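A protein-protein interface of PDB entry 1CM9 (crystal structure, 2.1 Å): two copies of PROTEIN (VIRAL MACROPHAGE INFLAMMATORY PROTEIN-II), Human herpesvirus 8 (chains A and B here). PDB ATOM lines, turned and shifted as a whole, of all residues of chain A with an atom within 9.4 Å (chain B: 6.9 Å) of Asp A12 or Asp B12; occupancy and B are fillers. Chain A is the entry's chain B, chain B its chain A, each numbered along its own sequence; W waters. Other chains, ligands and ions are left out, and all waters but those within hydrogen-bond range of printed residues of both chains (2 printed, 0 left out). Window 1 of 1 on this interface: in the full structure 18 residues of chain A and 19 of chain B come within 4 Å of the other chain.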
ATOM      1  N   HIS A   9     -23.342 -25.002  -7.825  1.00  0.00           N
ATOM      2  CA  HIS A   9     -23.462 -23.609  -7.426  1.00  0.00           C
ATOM      3  C   HIS A   9     -22.120 -22.892  -7.454  1.00  0.00           C
ATOM      4  O   HIS A   9     -21.297 -23.066  -6.561  1.00  0.00           O
ATOM      5  CB  HIS A   9     -24.058 -23.537  -6.023  1.00  0.00           C
ATOM      6  CG  HIS A   9     -25.456 -24.064  -5.937  1.00  0.00           C
ATOM      7  ND1 HIS A   9     -26.563 -23.281  -6.188  1.00  0.00           N
ATOM      8  CD2 HIS A   9     -25.927 -25.299  -5.648  1.00  0.00           C
ATOM      9  CE1 HIS A   9     -27.657 -24.011  -6.053  1.00  0.00           C
ATOM     10  NE2 HIS A   9     -27.297 -25.239  -5.725  1.00  0.00           N
ATOM     11  N   ARG A  10     -21.899 -22.091  -8.489  1.00  0.00           N
ATOM     12  CA  ARG A  10     -20.654 -21.340  -8.605  1.00  0.00           C
ATOM     13  C   ARG A  10     -20.683 -20.114  -7.711  1.00  0.00           C
ATOM     14  O   ARG A  10     -21.745 -19.599  -7.373  1.00  0.00           O
ATOM     15  CB  ARG A  10     -20.412 -20.906 -10.051  1.00  0.00           C
ATOM     16  CG  ARG A  10     -19.894 -22.022 -10.930  1.00  0.00           C
ATOM     17  CD  ARG A  10     -19.278 -21.501 -12.219  1.00  0.00           C
ATOM     18  NE  ARG A  10     -20.277 -21.073 -13.191  1.00  0.00           N
ATOM     19  CZ  ARG A  10     -19.989 -20.695 -14.434  1.00  0.00           C
ATOM     20  NH1 ARG A  10     -18.728 -20.693 -14.849  1.00  0.00           N
ATOM     21  NH2 ARG A  10     -20.957 -20.331 -15.264  1.00  0.00           N
ATOM     22  N   PRO A  11     -19.510 -19.632  -7.297  1.00  0.00           N
ATOM     23  CA  PRO A  11     -19.528 -18.450  -6.439  1.00  0.00           C
ATOM     24  C   PRO A  11     -19.818 -17.240  -7.327  1.00  0.00           C
ATOM     25  O   PRO A  11     -19.618 -17.301  -8.542  1.00  0.00           O
ATOM     26  CB  PRO A  11     -18.127 -18.451  -5.844  1.00  0.00           C
ATOM     27  CG  PRO A  11     -17.296 -18.954  -6.980  1.00  0.00           C
ATOM     28  CD  PRO A  11     -18.130 -20.080  -7.567  1.00  0.00           C
ATOM     29  N   ASP A  12     -20.311 -16.156  -6.739  1.00  0.00           N
ATOM     30  CA  ASP A  12     -20.607 -14.966  -7.527  1.00  0.00           C
ATOM     31  C   ASP A  12     -19.774 -13.792  -7.039  1.00  0.00           C
ATOM     32  O   ASP A  12     -19.361 -13.752  -5.890  1.00  0.00           O
ATOM     33  CB  ASP A  12     -22.100 -14.630  -7.466  1.00  0.00           C
ATOM     34  CG  ASP A  12     -22.552 -13.772  -8.648  1.00  0.00           C
ATOM     35  OD1 ASP A  12     -23.773 -13.733  -8.929  1.00  0.00           O
ATOM     36  OD2 ASP A  12     -21.689 -13.136  -9.302  1.00  0.00           O
ATOM     37  N   LYS A  13     -19.522 -12.840  -7.927  1.00  0.00           N
ATOM     38  CA  LYS A  13     -18.711 -11.682  -7.585  1.00  0.00           C
ATOM     39  C   LYS A  13     -19.496 -10.637  -6.826  1.00  0.00           C
ATOM     40  O   LYS A  13     -20.536 -10.177  -7.280  1.00  0.00           O
ATOM     41  CB  LYS A  13     -18.107 -11.078  -8.855  1.00  0.00           C
ATOM     42  CG  LYS A  13     -16.985 -11.924  -9.452  1.00  0.00           C
ATOM     43  CD  LYS A  13     -16.559 -11.431 -10.825  1.00  0.00           C
ATOM     44  CE  LYS A  13     -15.417 -12.278 -11.385  1.00  0.00           C
ATOM     45  NZ  LYS A  13     -15.161 -11.997 -12.829  1.00  0.00           N
ATOM     46  N   CYS A  14     -18.998 -10.288  -5.649  1.00  0.00           N
ATOM     47  CA  CYS A  14     -19.640  -9.286  -4.818  1.00  0.00           C
ATOM     48  C   CYS A  14     -18.622  -8.234  -4.399  1.00  0.00           C
ATOM     49  O   CYS A  14     -17.433  -8.517  -4.263  1.00  0.00           O
ATOM     50  CB  CYS A  14     -20.230  -9.914  -3.559  1.00  0.00           C
ATOM     51  SG  CYS A  14     -21.698 -10.981  -3.754  1.00  0.00           S
ATOM     52  N   CYS A  15     -19.098  -7.014  -4.197  1.00  0.00           N
ATOM     53  CA  CYS A  15     -18.226  -5.940  -3.769  1.00  0.00           C
ATOM     54  C   CYS A  15     -18.230  -5.872  -2.250  1.00  0.00           C
ATOM     55  O   CYS A  15     -19.269  -5.657  -1.626  1.00  0.00           O
ATOM     56  CB  CYS A  15     -18.677  -4.610  -4.377  1.00  0.00           C
ATOM     57  SG  CYS A  15     -18.332  -4.484  -6.162  1.00  0.00           S
ATOM     58  N   LEU A  16     -17.058  -6.092  -1.667  1.00  0.00           N
ATOM     59  CA  LEU A  16     -16.887  -6.056  -0.222  1.00  0.00           C
ATOM     60  C   LEU A  16     -16.208  -4.743   0.139  1.00  0.00           C
ATOM     61  O   LEU A  16     -16.241  -4.299   1.289  1.00  0.00           O
ATOM     62  CB  LEU A  16     -16.041  -7.252   0.231  1.00  0.00           C
ATOM     63  CG  LEU A  16     -16.770  -8.569   0.532  1.00  0.00           C
ATOM     64  CD1 LEU A  16     -17.977  -8.753  -0.365  1.00  0.00           C
ATOM     65  CD2 LEU A  16     -15.790  -9.712   0.372  1.00  0.00           C
ATOM     66  N   GLY A  17     -15.591  -4.132  -0.865  1.00  0.00           N
ATOM     67  CA  GLY A  17     -14.915  -2.861  -0.681  1.00  0.00           C
ATOM     68  C   GLY A  17     -15.260  -1.960  -1.847  1.00  0.00           C
ATOM     69  O   GLY A  17     -15.559  -2.446  -2.940  1.00  0.00           O
ATOM     70  N   TYR A  32     -20.519  -3.405 -14.838  1.00  0.00           N
ATOM     71  CA  TYR A  32     -21.412  -4.557 -14.682  1.00  0.00           C
ATOM     72  C   TYR A  32     -22.046  -4.588 -13.296  1.00  0.00           C
ATOM     73  O   TYR A  32     -21.391  -4.321 -12.301  1.00  0.00           O
ATOM     74  CB  TYR A  32     -20.614  -5.847 -14.907  1.00  0.00           C
ATOM     75  CG  TYR A  32     -21.441  -7.002 -15.408  1.00  0.00           C
ATOM     76  CD1 TYR A  32     -21.866  -8.015 -14.554  1.00  0.00           C
ATOM     77  CD2 TYR A  32     -21.781  -7.085 -16.748  1.00  0.00           C
ATOM     78  CE1 TYR A  32     -22.618  -9.098 -15.045  1.00  0.00           C
ATOM     79  CE2 TYR A  32     -22.515  -8.134 -17.241  1.00  0.00           C
ATOM     80  CZ  TYR A  32     -22.929  -9.141 -16.393  1.00  0.00           C
ATOM     81  OH  TYR A  32     -23.629 -10.186 -16.934  1.00  0.00           O
ATOM     82  N   PRO A  33     -23.336  -4.944 -13.211  1.00  0.00           N
ATOM     83  CA  PRO A  33     -23.954  -4.973 -11.883  1.00  0.00           C
ATOM     84  C   PRO A  33     -23.625  -6.239 -11.099  1.00  0.00           C
ATOM     85  O   PRO A  33     -23.239  -7.242 -11.685  1.00  0.00           O
ATOM     86  CB  PRO A  33     -25.435  -4.870 -12.205  1.00  0.00           C
ATOM     87  CG  PRO A  33     -25.542  -5.679 -13.470  1.00  0.00           C
ATOM     88  CD  PRO A  33     -24.306  -5.295 -14.266  1.00  0.00           C
ATOM     89  N   THR A  34     -23.732  -6.179  -9.775  1.00  0.00           N
ATOM     90  CA  THR A  34     -23.517  -7.364  -8.955  1.00  0.00           C
ATOM     91  C   THR A  34     -24.914  -7.865  -8.550  1.00  0.00           C
ATOM     92  O   THR A  34     -25.893  -7.135  -8.672  1.00  0.00           O
ATOM     93  CB  THR A  34     -22.697  -7.072  -7.684  1.00  0.00           C
ATOM     94  OG1 THR A  34     -23.230  -5.922  -7.013  1.00  0.00           O
ATOM     95  CG2 THR A  34     -21.218  -6.855  -8.031  1.00  0.00           C
ATOM     96  N   SER A  35     -25.006  -9.101  -8.066  1.00  0.00           N
ATOM     97  CA  SER A  35     -26.290  -9.693  -7.670  1.00  0.00           C
ATOM     98  C   SER A  35     -26.983  -8.948  -6.536  1.00  0.00           C
ATOM     99  O   SER A  35     -26.332  -8.548  -5.582  1.00  0.00           O
ATOM    100  CB  SER A  35     -26.068 -11.134  -7.213  1.00  0.00           C
ATOM    101  OG  SER A  35     -27.246 -11.659  -6.634  1.00  0.00           O
ATOM    102  N   GLN A  36     -28.301  -8.790  -6.610  1.00  0.00           N
ATOM    103  CA  GLN A  36     -29.014  -8.108  -5.532  1.00  0.00           C
ATOM    104  C   GLN A  36     -28.837  -8.884  -4.240  1.00  0.00           C
ATOM    105  O   GLN A  36     -29.072  -8.364  -3.163  1.00  0.00           O
ATOM    106  CB  GLN A  36     -30.513  -7.992  -5.808  1.00  0.00           C
ATOM    107  CG  GLN A  36     -30.910  -7.196  -7.034  1.00  0.00           C
ATOM    108  CD  GLN A  36     -31.114  -8.077  -8.240  1.00  0.00           C
ATOM    109  OE1 GLN A  36     -31.623  -7.635  -9.271  1.00  0.00           O
ATOM    110  NE2 GLN A  36     -30.716  -9.338  -8.121  1.00  0.00           N
ATOM    111  N   LEU A  37     -28.414 -10.136  -4.345  1.00  0.00           N
ATOM    112  CA  LEU A  37     -28.230 -10.955  -3.159  1.00  0.00           C
ATOM    113  C   LEU A  37     -26.920 -10.721  -2.415  1.00  0.00           C
ATOM    114  O   LEU A  37     -26.694 -11.309  -1.364  1.00  0.00           O
ATOM    115  CB  LEU A  37     -28.374 -12.418  -3.545  1.00  0.00           C
ATOM    116  CG  LEU A  37     -29.691 -12.660  -4.288  1.00  0.00           C
ATOM    117  CD1 LEU A  37     -29.778 -14.104  -4.751  1.00  0.00           C
ATOM    118  CD2 LEU A  37     -30.846 -12.303  -3.373  1.00  0.00           C
ATOM    119  N   CYS A  38     -26.056  -9.864  -2.956  1.00  0.00           N
ATOM    120  CA  CYS A  38     -24.781  -9.565  -2.302  1.00  0.00           C
ATOM    121  C   CYS A  38     -25.010  -8.666  -1.099  1.00  0.00           C
ATOM    122  O   CYS A  38     -25.947  -7.872  -1.082  1.00  0.00           O
ATOM    123  CB  CYS A  38     -23.825  -8.850  -3.253  1.00  0.00           C
ATOM    124  SG  CYS A  38     -23.130  -9.820  -4.628  1.00  0.00           S
ATOM    125  N   SER A  39     -24.135  -8.780  -0.105  1.00  0.00           N
ATOM    126  CA  SER A  39     -24.242  -7.988   1.110  1.00  0.00           C
ATOM    127  C   SER A  39     -24.422  -6.508   0.808  1.00  0.00           C
ATOM    128  O   SER A  39     -25.369  -5.882   1.289  1.00  0.00           O
ATOM    129  CB  SER A  39     -22.993  -8.168   1.972  1.00  0.00           C
ATOM    130  OG  SER A  39     -22.764  -9.531   2.247  1.00  0.00           O
ATOM    131  N   LYS A  40     -23.509  -5.954   0.014  1.00  0.00           N
ATOM    132  CA  LYS A  40     -23.562  -4.542  -0.336  1.00  0.00           C
ATOM    133  C   LYS A  40     -23.904  -4.303  -1.806  1.00  0.00           C
ATOM    134  O   LYS A  40     -23.429  -5.021  -2.692  1.00  0.00           O
ATOM    135  CB  LYS A  40     -22.222  -3.876  -0.009  1.00  0.00           C
ATOM    136  CG  LYS A  40     -21.827  -3.976   1.457  1.00  0.00           C
ATOM    137  CD  LYS A  40     -20.793  -2.919   1.847  1.00  0.00           C
ATOM    138  CE  LYS A  40     -19.423  -3.185   1.234  1.00  0.00           C
ATOM    139  NZ  LYS A  40     -18.774  -4.387   1.829  1.00  0.00           N
ATOM    140  N   ILE A  44     -19.310  -3.132 -10.918  1.00  0.00           N
ATOM    141  CA  ILE A  44     -17.926  -3.430 -11.193  1.00  0.00           C
ATOM    142  C   ILE A  44     -17.522  -2.765 -12.487  1.00  0.00           C
ATOM    143  O   ILE A  44     -18.137  -2.971 -13.530  1.00  0.00           O
ATOM    144  CB  ILE A  44     -17.716  -4.946 -11.325  1.00  0.00           C
ATOM    145  CG1 ILE A  44     -18.179  -5.643 -10.037  1.00  0.00           C
ATOM    146  CG2 ILE A  44     -16.262  -5.229 -11.628  1.00  0.00           C
ATOM    147  CD1 ILE A  44     -18.351  -7.122 -10.182  1.00  0.00           C
ATOM    148  N   GLN A  52     -10.608  -5.006 -12.904  1.00  0.00           N
ATOM    149  CA  GLN A  52     -11.954  -4.871 -12.356  1.00  0.00           C
ATOM    150  C   GLN A  52     -12.008  -4.123 -11.024  1.00  0.00           C
ATOM    151  O   GLN A  52     -11.535  -4.608 -10.003  1.00  0.00           O
ATOM    152  CB  GLN A  52     -12.579  -6.254 -12.197  1.00  0.00           C
ATOM    153  CG  GLN A  52     -12.852  -6.934 -13.519  1.00  0.00           C
ATOM    154  CD  GLN A  52     -13.244  -8.392 -13.369  1.00  0.00           C
ATOM    155  OE1 GLN A  52     -14.083  -8.741 -12.537  1.00  0.00           O
ATOM    156  NE2 GLN A  52     -12.642  -9.253 -14.187  1.00  0.00           N
ATOM    157  N   VAL A  53     -12.611  -2.944 -11.041  1.00  0.00           N
ATOM    158  CA  VAL A  53     -12.727  -2.125  -9.846  1.00  0.00           C
ATOM    159  C   VAL A  53     -14.149  -2.091  -9.306  1.00  0.00           C
ATOM    160  O   VAL A  53     -15.093  -1.861 -10.056  1.00  0.00           O
ATOM    161  CB  VAL A  53     -12.299  -0.668 -10.140  1.00  0.00           C
ATOM    162  CG1 VAL A  53     -12.336   0.156  -8.866  1.00  0.00           C
ATOM    163  CG2 VAL A  53     -10.925  -0.655 -10.771  1.00  0.00           C
ATOM    164  N   CYS A  54     -14.294  -2.307  -8.006  1.00  0.00           N
ATOM    165  CA  CYS A  54     -15.599  -2.272  -7.356  1.00  0.00           C
ATOM    166  C   CYS A  54     -15.942  -0.843  -6.975  1.00  0.00           C
ATOM    167  O   CYS A  54     -15.065  -0.089  -6.551  1.00  0.00           O
ATOM    168  CB  CYS A  54     -15.601  -3.128  -6.089  1.00  0.00           C
ATOM    169  SG  CYS A  54     -16.312  -4.786  -6.302  1.00  0.00           S
ATOM    170  N   HIS B   9      -9.096  -2.911  -6.290  1.00  0.00           N
ATOM    171  CA  HIS B   9     -10.075  -2.956  -5.211  1.00  0.00           C
ATOM    172  C   HIS B   9     -11.009  -4.092  -5.603  1.00  0.00           C
ATOM    173  O   HIS B   9     -12.138  -4.193  -5.128  1.00  0.00           O
ATOM    174  CB  HIS B   9     -10.860  -1.651  -5.134  1.00  0.00           C
ATOM    175  CG  HIS B   9     -11.320  -1.317  -3.754  1.00  0.00           C
ATOM    176  ND1 HIS B   9     -10.500  -0.714  -2.823  1.00  0.00           N
ATOM    177  CD2 HIS B   9     -12.497  -1.542  -3.124  1.00  0.00           C
ATOM    178  CE1 HIS B   9     -11.151  -0.584  -1.682  1.00  0.00           C
ATOM    179  NE2 HIS B   9     -12.365  -1.080  -1.838  1.00  0.00           N
ATOM    180  N   ARG B  10     -10.489  -4.929  -6.497  1.00  0.00           N
ATOM    181  CA  ARG B  10     -11.155  -6.094  -7.068  1.00  0.00           C
ATOM    182  C   ARG B  10     -12.316  -6.688  -6.282  1.00  0.00           C
ATOM    183  O   ARG B  10     -12.303  -6.709  -5.054  1.00  0.00           O
ATOM    184  CB  ARG B  10     -10.116  -7.183  -7.342  1.00  0.00           C
ATOM    185  N   PRO B  11     -13.343  -7.179  -6.996  1.00  0.00           N
ATOM    186  CA  PRO B  11     -14.526  -7.791  -6.385  1.00  0.00           C
ATOM    187  C   PRO B  11     -14.147  -9.152  -5.810  1.00  0.00           C
ATOM    188  O   PRO B  11     -13.213  -9.793  -6.291  1.00  0.00           O
ATOM    189  CB  PRO B  11     -15.488  -7.911  -7.555  1.00  0.00           C
ATOM    190  CG  PRO B  11     -14.568  -8.141  -8.710  1.00  0.00           C
ATOM    191  CD  PRO B  11     -13.489  -7.121  -8.461  1.00  0.00           C
ATOM    192  N   ASP B  12     -14.875  -9.590  -4.790  1.00  0.00           N
ATOM    193  CA  ASP B  12     -14.587 -10.867  -4.146  1.00  0.00           C
ATOM    194  C   ASP B  12     -15.577 -11.973  -4.507  1.00  0.00           C
ATOM    195  O   ASP B  12     -16.712 -11.711  -4.904  1.00  0.00           O
ATOM    196  CB  ASP B  12     -14.547 -10.680  -2.627  1.00  0.00           C
ATOM    197  N   LYS B  13     -15.126 -13.214  -4.368  1.00  0.00           N
ATOM    198  CA  LYS B  13     -15.960 -14.376  -4.649  1.00  0.00           C
ATOM    199  C   LYS B  13     -16.779 -14.687  -3.400  1.00  0.00           C
ATOM    200  O   LYS B  13     -16.231 -14.893  -2.320  1.00  0.00           O
ATOM    201  CB  LYS B  13     -15.089 -15.588  -5.011  1.00  0.00           C
ATOM    202  CG  LYS B  13     -14.402 -15.502  -6.370  1.00  0.00           C
ATOM    203  CD  LYS B  13     -15.419 -15.462  -7.502  1.00  0.00           C
ATOM    204  CE  LYS B  13     -14.745 -15.466  -8.866  1.00  0.00           C
ATOM    205  NZ  LYS B  13     -13.877 -16.667  -9.049  1.00  0.00           N
ATOM    206  N   CYS B  14     -18.094 -14.699  -3.545  1.00  0.00           N
ATOM    207  CA  CYS B  14     -18.970 -14.993  -2.424  1.00  0.00           C
ATOM    208  C   CYS B  14     -19.957 -16.073  -2.834  1.00  0.00           C
ATOM    209  O   CYS B  14     -20.233 -16.256  -4.013  1.00  0.00           O
ATOM    210  CB  CYS B  14     -19.747 -13.747  -1.984  1.00  0.00           C
ATOM    211  SG  CYS B  14     -18.822 -12.449  -1.097  1.00  0.00           S
ATOM    212  N   CYS B  15     -20.494 -16.777  -1.848  1.00  0.00           N
ATOM    213  CA  CYS B  15     -21.451 -17.844  -2.108  1.00  0.00           C
ATOM    214  C   CYS B  15     -22.889 -17.425  -1.840  1.00  0.00           C
ATOM    215  O   CYS B  15     -23.310 -17.296  -0.690  1.00  0.00           O
ATOM    216  CB  CYS B  15     -21.108 -19.066  -1.257  1.00  0.00           C
ATOM    217  SG  CYS B  15     -19.594 -19.921  -1.798  1.00  0.00           S
ATOM    218  N   LEU B  16     -23.651 -17.231  -2.904  1.00  0.00           N
ATOM    219  CA  LEU B  16     -25.036 -16.827  -2.743  1.00  0.00           C
ATOM    220  C   LEU B  16     -25.942 -18.050  -2.580  1.00  0.00           C
ATOM    221  O   LEU B  16     -27.011 -17.970  -1.979  1.00  0.00           O
ATOM    222  CB  LEU B  16     -25.469 -15.972  -3.937  1.00  0.00           C
ATOM    223  CG  LEU B  16     -24.570 -14.751  -4.179  1.00  0.00           C
ATOM    224  CD1 LEU B  16     -25.058 -13.992  -5.400  1.00  0.00           C
ATOM    225  CD2 LEU B  16     -24.566 -13.845  -2.955  1.00  0.00           C
ATOM    226  N   SER B  35     -14.422 -14.638   1.920  1.00  0.00           N
ATOM    227  CA  SER B  35     -14.316 -13.590   2.933  1.00  0.00           C
ATOM    228  C   SER B  35     -15.441 -13.692   3.960  1.00  0.00           C
ATOM    229  O   SER B  35     -16.529 -14.194   3.661  1.00  0.00           O
ATOM    230  CB  SER B  35     -14.361 -12.204   2.287  1.00  0.00           C
ATOM    231  OG  SER B  35     -14.371 -11.197   3.287  1.00  0.00           O
ATOM    232  N   CYS B  38     -18.643 -11.611   3.379  1.00  0.00           N
ATOM    233  CA  CYS B  38     -19.647 -12.047   2.424  1.00  0.00           C
ATOM    234  C   CYS B  38     -21.002 -12.191   3.098  1.00  0.00           C
ATOM    235  O   CYS B  38     -21.097 -12.330   4.315  1.00  0.00           O
ATOM    236  CB  CYS B  38     -19.266 -13.385   1.791  1.00  0.00           C
ATOM    237  SG  CYS B  38     -17.959 -13.359   0.519  1.00  0.00           S
ATOM    238  N   ILE B  44     -15.284 -22.611  -0.904  1.00  0.00           N
ATOM    239  CA  ILE B  44     -15.369 -22.921  -2.312  1.00  0.00           C
ATOM    240  C   ILE B  44     -14.480 -24.127  -2.558  1.00  0.00           C
ATOM    241  O   ILE B  44     -13.339 -24.173  -2.084  1.00  0.00           O
ATOM    242  CB  ILE B  44     -14.931 -21.727  -3.176  1.00  0.00           C
ATOM    243  CG1 ILE B  44     -15.945 -20.586  -3.010  1.00  0.00           C
ATOM    244  CG2 ILE B  44     -14.830 -22.148  -4.645  1.00  0.00           C
ATOM    245  CD1 ILE B  44     -15.559 -19.315  -3.728  1.00  0.00           C
ATOM    246  N   CYS B  54     -19.653 -23.848  -4.463  1.00  0.00           N
ATOM    247  CA  CYS B  54     -19.997 -23.287  -3.159  1.00  0.00           C
ATOM    248  C   CYS B  54     -20.631 -24.266  -2.180  1.00  0.00           C
ATOM    249  O   CYS B  54     -21.543 -25.018  -2.536  1.00  0.00           O
ATOM    250  CB  CYS B  54     -20.947 -22.112  -3.343  1.00  0.00           C
ATOM    251  SG  CYS B  54     -20.102 -20.545  -3.671  1.00  0.00           S
HETATM  252  O   HOH W   1     -21.714 -10.417  -0.272  1.00  0.00           O
HETATM  253  O   HOH W   2     -14.176  -5.757  -3.296  1.00  0.00           O
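Water W2 lies within hydrogen-bond range of O of Arg B10 (2.7 Å), O of His B9 (3.2 Å), N of Gly A17 (3.2 Å) and N of Leu A16 (3.3 Å). Water W1 lies within hydrogen-bond range of the side-chain hydroxyl (OG) of Ser A39, the side-chain sulfur (SG) of Cys A14 and the side-chain sulfur (SG) of Cys B14.
Hydrophobic or aromatic side chains of chain B within 4 Å of the printed part of chain A: His B9, Pro B11, Leu B16 and Ile B44. Among the printed residues, 25 pairs touch across the chains. Among the printed residues, no Asp or Glu carboxylate lies within 4 Å of a Lys or Arg side-chain nitrogen of the other chain.
O of Asp B12 is in hydrogen-bond range of N of Cys A14, 2.8 Å away. O of Cys B14 lies within hydrogen-bond range of N of Asp A12 (2.7 Å). The backbone carbonyl oxygen (O) of His A9 sits at hydrogen-bond distance from the backbone NH (N) of Cys B54, at 2.8 Å. The side-chain sulfur (SG) of Cys B54 sits close to the backbone nitrogen (N) of Pro A11, at 3.8 Å. The backbone carbonyl oxygen of Asp A12 sits close to the backbone carbonyl oxygen of Asp B12 (3.5 Å).
His A9 touches Cys B54, and with the chains exchanged Cys A54 touches His B9. Pro A11 touches Ile B44, and with the chains exchanged Ile A44 touches Pro B11. Asp A12 touches Lys B13, and with the chains exchanged Lys A13 touches Asp B12. Asp A12 touches Leu B16, and with the chains exchanged Leu A16 touches Asp B12. Positions printed for both chains: 9, 10, 11, 12, 13, 14, 15, 16, 35, 38, 44 and 54. Of the 25 pairs that touch across the chains among the printed residues, 18 have their exchanged pair printed and touching as well.
Among the printed residues, pairs that only touch across the chains: Gly A17 with His B9 (3.0 Å), Ser A39 with Cys B38 (3.3 Å), Gln A52 with Arg B10 (3.3 Å), Lys A13 with Asp B12 (3.3 Å), Pro A11 with Cys B14 (3.3 Å), Leu A16 with Asp B12 (3.4 Å), Ser A35 with Leu B16 (3.4 Å), Pro A11 with Ile B44 (3.4 Å), Leu A16 with Ser B35 (3.5 Å), Cys A54 with Pro B11 (3.5 Å), Gln A52 with Pro B11 (3.5 Å), Asp A12 with Leu B16 (3.7 Å), Cys A14 with Pro B11 (3.7 Å), Leu A37 with Leu B16 (3.7 Å), Asp A12 with Lys B13 (3.7 Å), Cys A54 with His B9 (3.7 Å), Cys A14 with Cys B14 (3.8 Å), Leu A16 with Cys B14 (3.9 Å), Ile A44 with Pro B11 (3.96 Å) and Pro A11 with Lys B13 (3.999 Å).
SG of Cys B54 forms a disulfide with SG of Cys B15 (2.0 Å). The side-chain amino group of Lys A13 sits at hydrogen-bond distance from the side-chain amide oxygen of Gln A52. SG of Cys A15 is disulfide-bonded to SG of Cys A54 (2.0 Å). The backbone carbonyl oxygen (O) of Leu A16 is in hydrogen-bond range of the side-chain amino group (NZ) of Lys A40. O of Ile A44 lies within hydrogen-bond range of N of Tyr A32, 2.8 Å away. The backbone NH (N) of Leu A37 lies close to the side-chain hydroxyl (OG) of Ser A35 (3.0 Å).
Printed residues of chain B within 4 Å of Asp A12: Asp B12, Lys B13, Cys B14 and Leu B16. Of chain A, only Asp A12, Lys A13, Cys A14 and Leu A16 come within 4 Å of Asp B12. Of chain A, only Cys A14, Ile A44, Gln A52 and Cys A54 come within 4 Å of Pro B11. Cys B14 touches four residues of chain A. Printed residues of chain B within 4 Å of His A9: Cys B54 (2.8 Å). Of the printed residues of chain B, Leu A16 touches Asp B12, Cys B14 and Ser B35. Printed residues of chain A within 4 Å of His B9: Gly A17 (3.0 Å) and Cys A54 (3.7 Å). Of the printed residues of chain A, Ser B35 touches Leu A16 (3.5 Å). Gln A36 touches none of the printed residues of chain B. Thr A34 touches none of the printed residues of chain B. The nearest printed residue of chain A that does not touch Cys B38 is Leu A16 (4.2 Å).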
